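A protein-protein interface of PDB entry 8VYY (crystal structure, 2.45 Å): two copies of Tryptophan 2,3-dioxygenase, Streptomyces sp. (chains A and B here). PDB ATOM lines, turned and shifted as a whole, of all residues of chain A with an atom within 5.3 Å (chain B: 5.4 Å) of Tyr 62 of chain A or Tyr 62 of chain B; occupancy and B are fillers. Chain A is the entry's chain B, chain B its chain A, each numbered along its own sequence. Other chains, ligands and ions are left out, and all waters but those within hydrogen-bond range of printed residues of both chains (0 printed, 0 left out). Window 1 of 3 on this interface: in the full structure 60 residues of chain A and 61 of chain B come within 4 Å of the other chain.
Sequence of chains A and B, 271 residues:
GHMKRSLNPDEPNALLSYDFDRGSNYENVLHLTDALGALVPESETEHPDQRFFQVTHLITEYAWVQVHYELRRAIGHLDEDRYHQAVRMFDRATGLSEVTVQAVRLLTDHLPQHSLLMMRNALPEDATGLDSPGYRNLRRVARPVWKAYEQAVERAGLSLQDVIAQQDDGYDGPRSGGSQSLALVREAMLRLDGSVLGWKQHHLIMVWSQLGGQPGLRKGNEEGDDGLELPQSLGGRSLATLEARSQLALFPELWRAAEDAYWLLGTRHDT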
ATOM      1  N   ALA A  35      24.884 -10.790   3.142  1.00  0.00           N
ATOM      2  CA  ALA A  35      25.384 -12.035   3.716  1.00  0.00           C
ATOM      3  C   ALA A  35      26.429 -11.768   4.797  1.00  0.00           C
ATOM      4  O   ALA A  35      26.388 -12.368   5.879  1.00  0.00           O
ATOM      5  CB  ALA A  35      25.952 -12.922   2.607  1.00  0.00           C
ATOM      6  N   LEU A  36      27.387 -10.880   4.520  1.00  0.00           N
ATOM      7  CA  LEU A  36      28.381 -10.536   5.526  1.00  0.00           C
ATOM      8  C   LEU A  36      27.765  -9.793   6.711  1.00  0.00           C
ATOM      9  O   LEU A  36      28.350  -9.787   7.802  1.00  0.00           O
ATOM     10  CB  LEU A  36      29.495  -9.707   4.887  1.00  0.00           C
ATOM     11  CG  LEU A  36      30.343 -10.437   3.840  1.00  0.00           C
ATOM     12  CD1 LEU A  36      31.358  -9.494   3.202  1.00  0.00           C
ATOM     13  CD2 LEU A  36      31.043 -11.629   4.464  1.00  0.00           C
ATOM     14  N   ALA A  38      25.332 -10.782   8.410  1.00  0.00           N
ATOM     15  CA  ALA A  38      24.840 -11.729   9.398  1.00  0.00           C
ATOM     16  C   ALA A  38      25.900 -12.124  10.428  1.00  0.00           C
ATOM     17  O   ALA A  38      25.549 -12.605  11.509  1.00  0.00           O
ATOM     18  CB  ALA A  38      24.282 -12.965   8.685  1.00  0.00           C
ATOM     19  N   LEU A  39      27.179 -11.915  10.141  1.00  0.00           N
ATOM     20  CA  LEU A  39      28.212 -12.312  11.089  1.00  0.00           C
ATOM     21  C   LEU A  39      28.084 -11.520  12.384  1.00  0.00           C
ATOM     22  O   LEU A  39      27.849 -10.307  12.362  1.00  0.00           O
ATOM     23  CB  LEU A  39      29.594 -12.109  10.465  1.00  0.00           C
ATOM     24  CG  LEU A  39      29.760 -12.905   9.162  1.00  0.00           C
ATOM     25  CD1 LEU A  39      31.119 -12.706   8.550  1.00  0.00           C
ATOM     26  CD2 LEU A  39      29.510 -14.378   9.391  1.00  0.00           C
ATOM     27  N   VAL A  55      30.157 -19.498  11.331  1.00  0.00           N
ATOM     28  CA  VAL A  55      30.353 -19.573   9.886  1.00  0.00           C
ATOM     29  C   VAL A  55      30.134 -20.990   9.375  1.00  0.00           C
ATOM     30  O   VAL A  55      29.593 -21.182   8.277  1.00  0.00           O
ATOM     31  CB  VAL A  55      31.748 -19.032   9.516  1.00  0.00           C
ATOM     32  CG1 VAL A  55      32.216 -19.567   8.181  1.00  0.00           C
ATOM     33  CG2 VAL A  55      31.698 -17.522   9.464  1.00  0.00           C
ATOM     34  N   HIS A  57      28.033 -23.183  10.559  1.00  0.00           N
ATOM     35  CA  HIS A  57      26.583 -23.350  10.461  1.00  0.00           C
ATOM     36  C   HIS A  57      26.031 -22.673   9.210  1.00  0.00           C
ATOM     37  O   HIS A  57      25.172 -23.235   8.514  1.00  0.00           O
ATOM     38  CB  HIS A  57      25.880 -22.771  11.688  1.00  0.00           C
ATOM     39  CG  HIS A  57      25.918 -23.654  12.890  1.00  0.00           C
ATOM     40  ND1 HIS A  57      27.027 -23.754  13.703  1.00  0.00           N
ATOM     41  CD2 HIS A  57      24.982 -24.475  13.423  1.00  0.00           C
ATOM     42  CE1 HIS A  57      26.771 -24.597  14.688  1.00  0.00           C
ATOM     43  NE2 HIS A  57      25.540 -25.055  14.537  1.00  0.00           N
ATOM     44  N   LEU A  58      26.482 -21.444   8.935  1.00  0.00           N
ATOM     45  CA  LEU A  58      25.940 -20.695   7.810  1.00  0.00           C
ATOM     46  C   LEU A  58      26.287 -21.367   6.491  1.00  0.00           C
ATOM     47  O   LEU A  58      25.431 -21.500   5.607  1.00  0.00           O
ATOM     48  CB  LEU A  58      26.456 -19.258   7.837  1.00  0.00           C
ATOM     49  CG  LEU A  58      25.973 -18.400   9.007  1.00  0.00           C
ATOM     50  CD1 LEU A  58      26.416 -16.975   8.809  1.00  0.00           C
ATOM     51  CD2 LEU A  58      24.462 -18.470   9.194  1.00  0.00           C
ATOM     52  N   ILE A  59      27.530 -21.821   6.348  1.00  0.00           N
ATOM     53  CA  ILE A  59      27.910 -22.567   5.153  1.00  0.00           C
ATOM     54  C   ILE A  59      27.013 -23.788   4.976  1.00  0.00           C
ATOM     55  O   ILE A  59      26.526 -24.064   3.876  1.00  0.00           O
ATOM     56  CB  ILE A  59      29.396 -22.950   5.235  1.00  0.00           C
ATOM     57  CG1 ILE A  59      30.235 -21.709   4.928  1.00  0.00           C
ATOM     58  CG2 ILE A  59      29.706 -24.119   4.309  1.00  0.00           C
ATOM     59  CD1 ILE A  59      31.701 -21.876   5.201  1.00  0.00           C
ATOM     60  N   THR A  60      26.745 -24.509   6.064  1.00  0.00           N
ATOM     61  CA  THR A  60      25.862 -25.664   5.985  1.00  0.00           C
ATOM     62  C   THR A  60      24.467 -25.256   5.558  1.00  0.00           C
ATOM     63  O   THR A  60      23.872 -25.877   4.664  1.00  0.00           O
ATOM     64  CB  THR A  60      25.795 -26.381   7.335  1.00  0.00           C
ATOM     65  OG1 THR A  60      27.091 -26.871   7.669  1.00  0.00           O
ATOM     66  CG2 THR A  60      24.816 -27.545   7.261  1.00  0.00           C
ATOM     67  N   GLU A  61      23.913 -24.221   6.201  1.00  0.00           N
ATOM     68  CA  GLU A  61      22.546 -23.843   5.878  1.00  0.00           C
ATOM     69  C   GLU A  61      22.442 -23.378   4.428  1.00  0.00           C
ATOM     70  O   GLU A  61      21.467 -23.693   3.742  1.00  0.00           O
ATOM     71  CB  GLU A  61      22.033 -22.787   6.856  1.00  0.00           C
ATOM     72  CG  GLU A  61      21.831 -23.319   8.314  1.00  0.00           C
ATOM     73  CD  GLU A  61      20.652 -24.306   8.510  1.00  0.00           C
ATOM     74  OE1 GLU A  61      19.745 -24.393   7.652  1.00  0.00           O
ATOM     75  OE2 GLU A  61      20.616 -24.995   9.555  1.00  0.00           O
ATOM     76  N   TYR A  62      23.464 -22.681   3.921  1.00  0.00           N
ATOM     77  CA  TYR A  62      23.455 -22.304   2.510  1.00  0.00           C
ATOM     78  C   TYR A  62      23.468 -23.528   1.608  1.00  0.00           C
ATOM     79  O   TYR A  62      22.758 -23.573   0.597  1.00  0.00           O
ATOM     80  CB  TYR A  62      24.645 -21.410   2.185  1.00  0.00           C
ATOM     81  CG  TYR A  62      24.347 -19.945   2.322  1.00  0.00           C
ATOM     82  CD1 TYR A  62      23.107 -19.431   1.998  1.00  0.00           C
ATOM     83  CD2 TYR A  62      25.302 -19.078   2.791  1.00  0.00           C
ATOM     84  CE1 TYR A  62      22.838 -18.081   2.143  1.00  0.00           C
ATOM     85  CE2 TYR A  62      25.039 -17.744   2.926  1.00  0.00           C
ATOM     86  CZ  TYR A  62      23.824 -17.251   2.611  1.00  0.00           C
ATOM     87  OH  TYR A  62      23.623 -15.908   2.770  1.00  0.00           O
ATOM     88  N   ALA A  63      24.281 -24.525   1.935  1.00  0.00           N
ATOM     89  CA  ALA A  63      24.304 -25.709   1.084  1.00  0.00           C
ATOM     90  C   ALA A  63      22.969 -26.448   1.135  1.00  0.00           C
ATOM     91  O   ALA A  63      22.471 -26.922   0.101  1.00  0.00           O
ATOM     92  CB  ALA A  63      25.461 -26.625   1.483  1.00  0.00           C
ATOM     93  N   TRP A  64      22.355 -26.518   2.321  1.00  0.00           N
ATOM     94  CA  TRP A  64      21.095 -27.245   2.460  1.00  0.00           C
ATOM     95  C   TRP A  64      19.951 -26.538   1.739  1.00  0.00           C
ATOM     96  O   TRP A  64      19.060 -27.202   1.183  1.00  0.00           O
ATOM     97  CB  TRP A  64      20.751 -27.450   3.941  1.00  0.00           C
ATOM     98  CG  TRP A  64      21.410 -28.669   4.536  1.00  0.00           C
ATOM     99  CD1 TRP A  64      21.913 -29.740   3.860  1.00  0.00           C
ATOM    100  CD2 TRP A  64      21.632 -28.935   5.930  1.00  0.00           C
ATOM    101  NE1 TRP A  64      22.437 -30.652   4.741  1.00  0.00           N
ATOM    102  CE2 TRP A  64      22.273 -30.184   6.017  1.00  0.00           C
ATOM    103  CE3 TRP A  64      21.338 -28.239   7.110  1.00  0.00           C
ATOM    104  CZ2 TRP A  64      22.640 -30.750   7.236  1.00  0.00           C
ATOM    105  CZ3 TRP A  64      21.689 -28.797   8.312  1.00  0.00           C
ATOM    106  CH2 TRP A  64      22.335 -30.044   8.373  1.00  0.00           C
ATOM    107  N   VAL A  65      19.935 -25.200   1.747  1.00  0.00           N
ATOM    108  CA  VAL A  65      18.847 -24.535   1.032  1.00  0.00           C
ATOM    109  C   VAL A  65      19.016 -24.766  -0.463  1.00  0.00           C
ATOM    110  O   VAL A  65      18.037 -24.999  -1.181  1.00  0.00           O
ATOM    111  CB  VAL A  65      18.751 -23.036   1.400  1.00  0.00           C
ATOM    112  CG1 VAL A  65      19.972 -22.276   0.931  1.00  0.00           C
ATOM    113  CG2 VAL A  65      17.499 -22.420   0.782  1.00  0.00           C
ATOM    114  N   GLN A  66      20.256 -24.824  -0.937  1.00  0.00           N
ATOM    115  CA  GLN A  66      20.485 -25.134  -2.341  1.00  0.00           C
ATOM    116  C   GLN A  66      20.131 -26.577  -2.670  1.00  0.00           C
ATOM    117  O   GLN A  66      19.647 -26.859  -3.772  1.00  0.00           O
ATOM    118  CB  GLN A  66      21.932 -24.849  -2.708  1.00  0.00           C
ATOM    119  CG  GLN A  66      22.184 -24.780  -4.195  1.00  0.00           C
ATOM    120  CD  GLN A  66      21.218 -23.843  -4.917  1.00  0.00           C
ATOM    121  OE1 GLN A  66      20.854 -22.776  -4.400  1.00  0.00           O
ATOM    122  NE2 GLN A  66      20.799 -24.243  -6.116  1.00  0.00           N
ATOM    123  N   VAL A  67      20.391 -27.513  -1.747  1.00  0.00           N
ATOM    124  CA  VAL A  67      19.986 -28.903  -1.976  1.00  0.00           C
ATOM    125  C   VAL A  67      18.477 -28.973  -2.161  1.00  0.00           C
ATOM    126  O   VAL A  67      17.972 -29.621  -3.086  1.00  0.00           O
ATOM    127  CB  VAL A  67      20.442 -29.816  -0.815  1.00  0.00           C
ATOM    128  CG1 VAL A  67      19.771 -31.192  -0.906  1.00  0.00           C
ATOM    129  CG2 VAL A  67      21.953 -29.990  -0.807  1.00  0.00           C
ATOM    130  N   ALA B  35      21.091 -14.135   6.964  1.00  0.00           N
ATOM    131  CA  ALA B  35      21.949 -14.745   5.955  1.00  0.00           C
ATOM    132  C   ALA B  35      21.133 -15.294   4.785  1.00  0.00           C
ATOM    133  O   ALA B  35      21.520 -15.131   3.620  1.00  0.00           O
ATOM    134  CB  ALA B  35      22.822 -15.831   6.597  1.00  0.00           C
ATOM    135  N   LEU B  36      19.997 -15.940   5.066  1.00  0.00           N
ATOM    136  CA  LEU B  36      19.165 -16.449   3.983  1.00  0.00           C
ATOM    137  C   LEU B  36      18.519 -15.322   3.200  1.00  0.00           C
ATOM    138  O   LEU B  36      18.186 -15.515   2.025  1.00  0.00           O
ATOM    139  CB  LEU B  36      18.093 -17.391   4.527  1.00  0.00           C
ATOM    140  CG  LEU B  36      18.679 -18.617   5.224  1.00  0.00           C
ATOM    141  CD1 LEU B  36      17.607 -19.445   5.909  1.00  0.00           C
ATOM    142  CD2 LEU B  36      19.469 -19.439   4.231  1.00  0.00           C
ATOM    143  N   ALA B  38      19.918 -12.882   1.909  1.00  0.00           N
ATOM    144  CA  ALA B  38      20.777 -12.510   0.791  1.00  0.00           C
ATOM    145  C   ALA B  38      20.529 -13.339  -0.463  1.00  0.00           C
ATOM    146  O   ALA B  38      20.976 -12.939  -1.545  1.00  0.00           O
ATOM    147  CB  ALA B  38      22.253 -12.625   1.190  1.00  0.00           C
ATOM    148  N   LEU B  39      19.838 -14.469  -0.359  1.00  0.00           N
ATOM    149  CA  LEU B  39      19.590 -15.266  -1.550  1.00  0.00           C
ATOM    150  C   LEU B  39      18.707 -14.490  -2.519  1.00  0.00           C
ATOM    151  O   LEU B  39      17.791 -13.773  -2.107  1.00  0.00           O
ATOM    152  CB  LEU B  39      18.959 -16.610  -1.177  1.00  0.00           C
ATOM    153  CG  LEU B  39      19.901 -17.531  -0.397  1.00  0.00           C
ATOM    154  CD1 LEU B  39      19.235 -18.850  -0.088  1.00  0.00           C
ATOM    155  CD2 LEU B  39      21.204 -17.753  -1.141  1.00  0.00           C
ATOM    156  N   VAL B  55      25.195 -19.287  -4.554  1.00  0.00           N
ATOM    157  CA  VAL B  55      25.490 -19.961  -3.290  1.00  0.00           C
ATOM    158  C   VAL B  55      26.943 -20.432  -3.222  1.00  0.00           C
ATOM    159  O   VAL B  55      27.567 -20.362  -2.153  1.00  0.00           O
ATOM    160  CB  VAL B  55      24.499 -21.120  -3.061  1.00  0.00           C
ATOM    161  CG1 VAL B  55      24.995 -22.034  -1.981  1.00  0.00           C
ATOM    162  CG2 VAL B  55      23.126 -20.567  -2.675  1.00  0.00           C
ATOM    163  N   HIS B  57      29.512 -18.917  -4.525  1.00  0.00           N
ATOM    164  CA  HIS B  57      30.275 -17.705  -4.193  1.00  0.00           C
ATOM    165  C   HIS B  57      30.120 -17.364  -2.723  1.00  0.00           C
ATOM    166  O   HIS B  57      31.097 -17.038  -2.044  1.00  0.00           O
ATOM    167  CB  HIS B  57      29.819 -16.497  -5.022  1.00  0.00           C
ATOM    168  CG  HIS B  57      30.310 -16.488  -6.435  1.00  0.00           C
ATOM    169  ND1 HIS B  57      29.630 -17.107  -7.463  1.00  0.00           N
ATOM    170  CD2 HIS B  57      31.392 -15.898  -7.000  1.00  0.00           C
ATOM    171  CE1 HIS B  57      30.286 -16.923  -8.596  1.00  0.00           C
ATOM    172  NE2 HIS B  57      31.358 -16.192  -8.341  1.00  0.00           N
ATOM    173  N   LEU B  58      28.884 -17.402  -2.224  1.00  0.00           N
ATOM    174  CA  LEU B  58      28.637 -17.008  -0.840  1.00  0.00           C
ATOM    175  C   LEU B  58      29.355 -17.939   0.135  1.00  0.00           C
ATOM    176  O   LEU B  58      29.958 -17.487   1.117  1.00  0.00           O
ATOM    177  CB  LEU B  58      27.128 -16.990  -0.573  1.00  0.00           C
ATOM    178  CG  LEU B  58      26.390 -15.809  -1.229  1.00  0.00           C
ATOM    179  CD1 LEU B  58      24.925 -15.805  -0.863  1.00  0.00           C
ATOM    180  CD2 LEU B  58      27.035 -14.486  -0.849  1.00  0.00           C
ATOM    181  N   ILE B  59      29.291 -19.244  -0.122  1.00  0.00           N
ATOM    182  CA  ILE B  59      30.010 -20.199   0.704  1.00  0.00           C
ATOM    183  C   ILE B  59      31.496 -19.881   0.690  1.00  0.00           C
ATOM    184  O   ILE B  59      32.158 -19.882   1.739  1.00  0.00           O
ATOM    185  CB  ILE B  59      29.723 -21.631   0.218  1.00  0.00           C
ATOM    186  CG1 ILE B  59      28.308 -22.045   0.636  1.00  0.00           C
ATOM    187  CG2 ILE B  59      30.768 -22.578   0.739  1.00  0.00           C
ATOM    188  CD1 ILE B  59      27.810 -23.384  -0.007  1.00  0.00           C
ATOM    189  N   THR B  60      32.029 -19.570  -0.498  1.00  0.00           N
ATOM    190  CA  THR B  60      33.440 -19.222  -0.626  1.00  0.00           C
ATOM    191  C   THR B  60      33.781 -17.985   0.180  1.00  0.00           C
ATOM    192  O   THR B  60      34.823 -17.938   0.859  1.00  0.00           O
ATOM    193  CB  THR B  60      33.794 -19.000  -2.094  1.00  0.00           C
ATOM    194  OG1 THR B  60      33.625 -20.231  -2.814  1.00  0.00           O
ATOM    195  CG2 THR B  60      35.212 -18.530  -2.218  1.00  0.00           C
ATOM    196  N   GLU B  61      32.906 -16.978   0.134  1.00  0.00           N
ATOM    197  CA  GLU B  61      33.222 -15.713   0.785  1.00  0.00           C
ATOM    198  C   GLU B  61      33.151 -15.850   2.301  1.00  0.00           C
ATOM    199  O   GLU B  61      33.946 -15.235   3.025  1.00  0.00           O
ATOM    200  CB  GLU B  61      32.279 -14.611   0.272  1.00  0.00           C
ATOM    201  CG  GLU B  61      32.547 -14.209  -1.207  1.00  0.00           C
ATOM    202  CD  GLU B  61      33.845 -13.391  -1.443  1.00  0.00           C
ATOM    203  OE1 GLU B  61      34.441 -12.833  -0.485  1.00  0.00           O
ATOM    204  OE2 GLU B  61      34.267 -13.301  -2.620  1.00  0.00           O
ATOM    205  N   TYR B  62      32.207 -16.654   2.797  1.00  0.00           N
ATOM    206  CA  TYR B  62      32.163 -16.938   4.227  1.00  0.00           C
ATOM    207  C   TYR B  62      33.433 -17.638   4.670  1.00  0.00           C
ATOM    208  O   TYR B  62      34.006 -17.322   5.715  1.00  0.00           O
ATOM    209  CB  TYR B  62      30.954 -17.805   4.552  1.00  0.00           C
ATOM    210  CG  TYR B  62      29.690 -17.049   4.828  1.00  0.00           C
ATOM    211  CD1 TYR B  62      29.714 -15.820   5.455  1.00  0.00           C
ATOM    212  CD2 TYR B  62      28.462 -17.567   4.466  1.00  0.00           C
ATOM    213  CE1 TYR B  62      28.542 -15.131   5.718  1.00  0.00           C
ATOM    214  CE2 TYR B  62      27.296 -16.881   4.727  1.00  0.00           C
ATOM    215  CZ  TYR B  62      27.337 -15.671   5.352  1.00  0.00           C
ATOM    216  OH  TYR B  62      26.162 -15.007   5.608  1.00  0.00           O
ATOM    217  N   ALA B  63      33.910 -18.578   3.872  1.00  0.00           N
ATOM    218  CA  ALA B  63      35.141 -19.246   4.244  1.00  0.00           C
ATOM    219  C   ALA B  63      36.303 -18.249   4.291  1.00  0.00           C
ATOM    220  O   ALA B  63      37.107 -18.271   5.235  1.00  0.00           O
ATOM    221  CB  ALA B  63      35.398 -20.421   3.285  1.00  0.00           C
ATOM    222  N   TRP B  64      36.393 -17.342   3.305  1.00  0.00           N
ATOM    223  CA  TRP B  64      37.556 -16.444   3.235  1.00  0.00           C
ATOM    224  C   TRP B  64      37.527 -15.396   4.346  1.00  0.00           C
ATOM    225  O   TRP B  64      38.581 -15.034   4.896  1.00  0.00           O
ATOM    226  CB  TRP B  64      37.636 -15.769   1.866  1.00  0.00           C
ATOM    227  CG  TRP B  64      38.333 -16.592   0.823  1.00  0.00           C
ATOM    228  CD1 TRP B  64      39.244 -17.597   1.036  1.00  0.00           C
ATOM    229  CD2 TRP B  64      38.180 -16.486  -0.597  1.00  0.00           C
ATOM    230  NE1 TRP B  64      39.661 -18.118  -0.164  1.00  0.00           N
ATOM    231  CE2 TRP B  64      39.023 -17.459  -1.182  1.00  0.00           C
ATOM    232  CE3 TRP B  64      37.404 -15.672  -1.433  1.00  0.00           C
ATOM    233  CZ2 TRP B  64      39.117 -17.632  -2.565  1.00  0.00           C
ATOM    234  CZ3 TRP B  64      37.500 -15.842  -2.803  1.00  0.00           C
ATOM    235  CH2 TRP B  64      38.352 -16.814  -3.359  1.00  0.00           C
ATOM    236  N   VAL B  65      36.334 -14.902   4.706  1.00  0.00           N
ATOM    237  CA  VAL B  65      36.284 -13.934   5.799  1.00  0.00           C
ATOM    238  C   VAL B  65      36.731 -14.594   7.092  1.00  0.00           C
ATOM    239  O   VAL B  65      37.413 -13.974   7.923  1.00  0.00           O
ATOM    240  CB  VAL B  65      34.880 -13.305   5.929  1.00  0.00           C
ATOM    241  CG1 VAL B  65      33.840 -14.357   6.201  1.00  0.00           C
ATOM    242  CG2 VAL B  65      34.869 -12.267   7.059  1.00  0.00           C
ATOM    243  N   GLN B  66      36.417 -15.880   7.256  1.00  0.00           N
ATOM    244  CA  GLN B  66      36.844 -16.605   8.444  1.00  0.00           C
ATOM    245  C   GLN B  66      38.346 -16.891   8.420  1.00  0.00           C
ATOM    246  O   GLN B  66      39.005 -16.847   9.467  1.00  0.00           O
ATOM    247  CB  GLN B  66      36.024 -17.892   8.575  1.00  0.00           C
ATOM    248  CG  GLN B  66      36.112 -18.544   9.941  1.00  0.00           C
ATOM    249  CD  GLN B  66      35.775 -17.577  11.058  1.00  0.00           C
ATOM    250  OE1 GLN B  66      34.852 -16.771  10.933  1.00  0.00           O
ATOM    251  NE2 GLN B  66      36.528 -17.645  12.153  1.00  0.00           N
ATOM    252  N   VAL B  67      38.900 -17.222   7.249  1.00  0.00           N
ATOM    253  CA  VAL B  67      40.357 -17.348   7.116  1.00  0.00           C
ATOM    254  C   VAL B  67      41.048 -16.084   7.628  1.00  0.00           C
ATOM    255  O   VAL B  67      42.007 -16.136   8.412  1.00  0.00           O
ATOM    256  CB  VAL B  67      40.740 -17.623   5.645  1.00  0.00           C
ATOM    257  CG1 VAL B  67      42.209 -17.323   5.401  1.00  0.00           C
ATOM    258  CG2 VAL B  67      40.435 -19.058   5.234  1.00  0.00           C
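Ala 35 of chain A touches Leu 58 of chain B, but with the chains exchanged Leu 58 of chain A does not touch Ala 35 of chain B (4.05 Å).
Ala 35 of chain A touches Tyr 62 of chain B, and with the chains exchanged Tyr 62 of chain A touches Ala 35 of chain B.
Leu 39 of chain A touches Tyr 62 of chain B, and with the chains exchanged Tyr 62 of chain A touches Leu 39 of chain B.
Val 55 of chain A touches Tyr 62 of chain B, and with the chains exchanged Tyr 62 of chain A touches Val 55 of chain B.
OH of Tyr 62 of chain B sits at hydrogen-bond distance from O of Ala 35 of chain A, at 2.7 Å.
O of Ala 35 of chain B sits close to OH of Tyr 62 of chain A (2.4 Å).
Ala 35 of chain A touches Leu 58 of chain B.
Leu 39 of chain A touches Tyr 62 of chain B.
Val 65 of chain B touches Leu 39 of chain A.
Val 55 of chain A touches Tyr 62 of chain B.
OE1 of Gln 66 of chain B touches CG2 of Val 55 of chain A, 3.6 Å away.
CG1 of Ile 59 of chain A touches CB of Tyr 62 of chain B (3.99 Å).
OH of Tyr 62 of chain A touches CB of Ala 38 of chain B, 3.9 Å away.
Leu 39 of chain B touches Tyr 62 of chain A.
Tyr 62 of chain A touches Leu 58 of chain B (OH to CD1, 3.9 Å).
Tyr 62 of chain A touches Tyr 62 of chain B.
Printed residues of chain B within 4 Å of Ala 35 of chain A: Ala 38, Leu 58 and Tyr 62.
Of the printed residues of chain B, Val 55 of chain A touches Tyr 62 and Gln 66.
Of the printed residues of chain B, Leu 58 of chain A touches Tyr 62 (3.8 Å).
Ala 63 of chain A touches none of the printed residues of chain B.
Printed residues of chain A within 4 Å of Tyr 62 of chain B: Ala 35, Leu 39, Val 55, Leu 58, Ile 59 and Tyr 62.
The nearest printed residue of chain A that does not touch Tyr 62 of chain B is Ala 38 of chain A (4.1 Å).
The nearest printed residue of chain B that does not touch Val 55 of chain A is Ala 63 of chain B (4.7 Å).
Of the 16 printed residues of chain A, 9 touch a printed residue of chain B.
Hydrophobic or aromatic side chains of chain A that line the printed part of chain B: Ala 35, Ala 38, Leu 39, Val 55, Leu 58, Ile 59, Tyr 62 and Val 65.
Along chain A the printed residues that touch a printed residue of chain B span positions 35 to 66.
Among the printed residues, no Asp or Glu carboxylate lies within 4 Å of a Lys or Arg side-chain nitrogen of the other chain.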
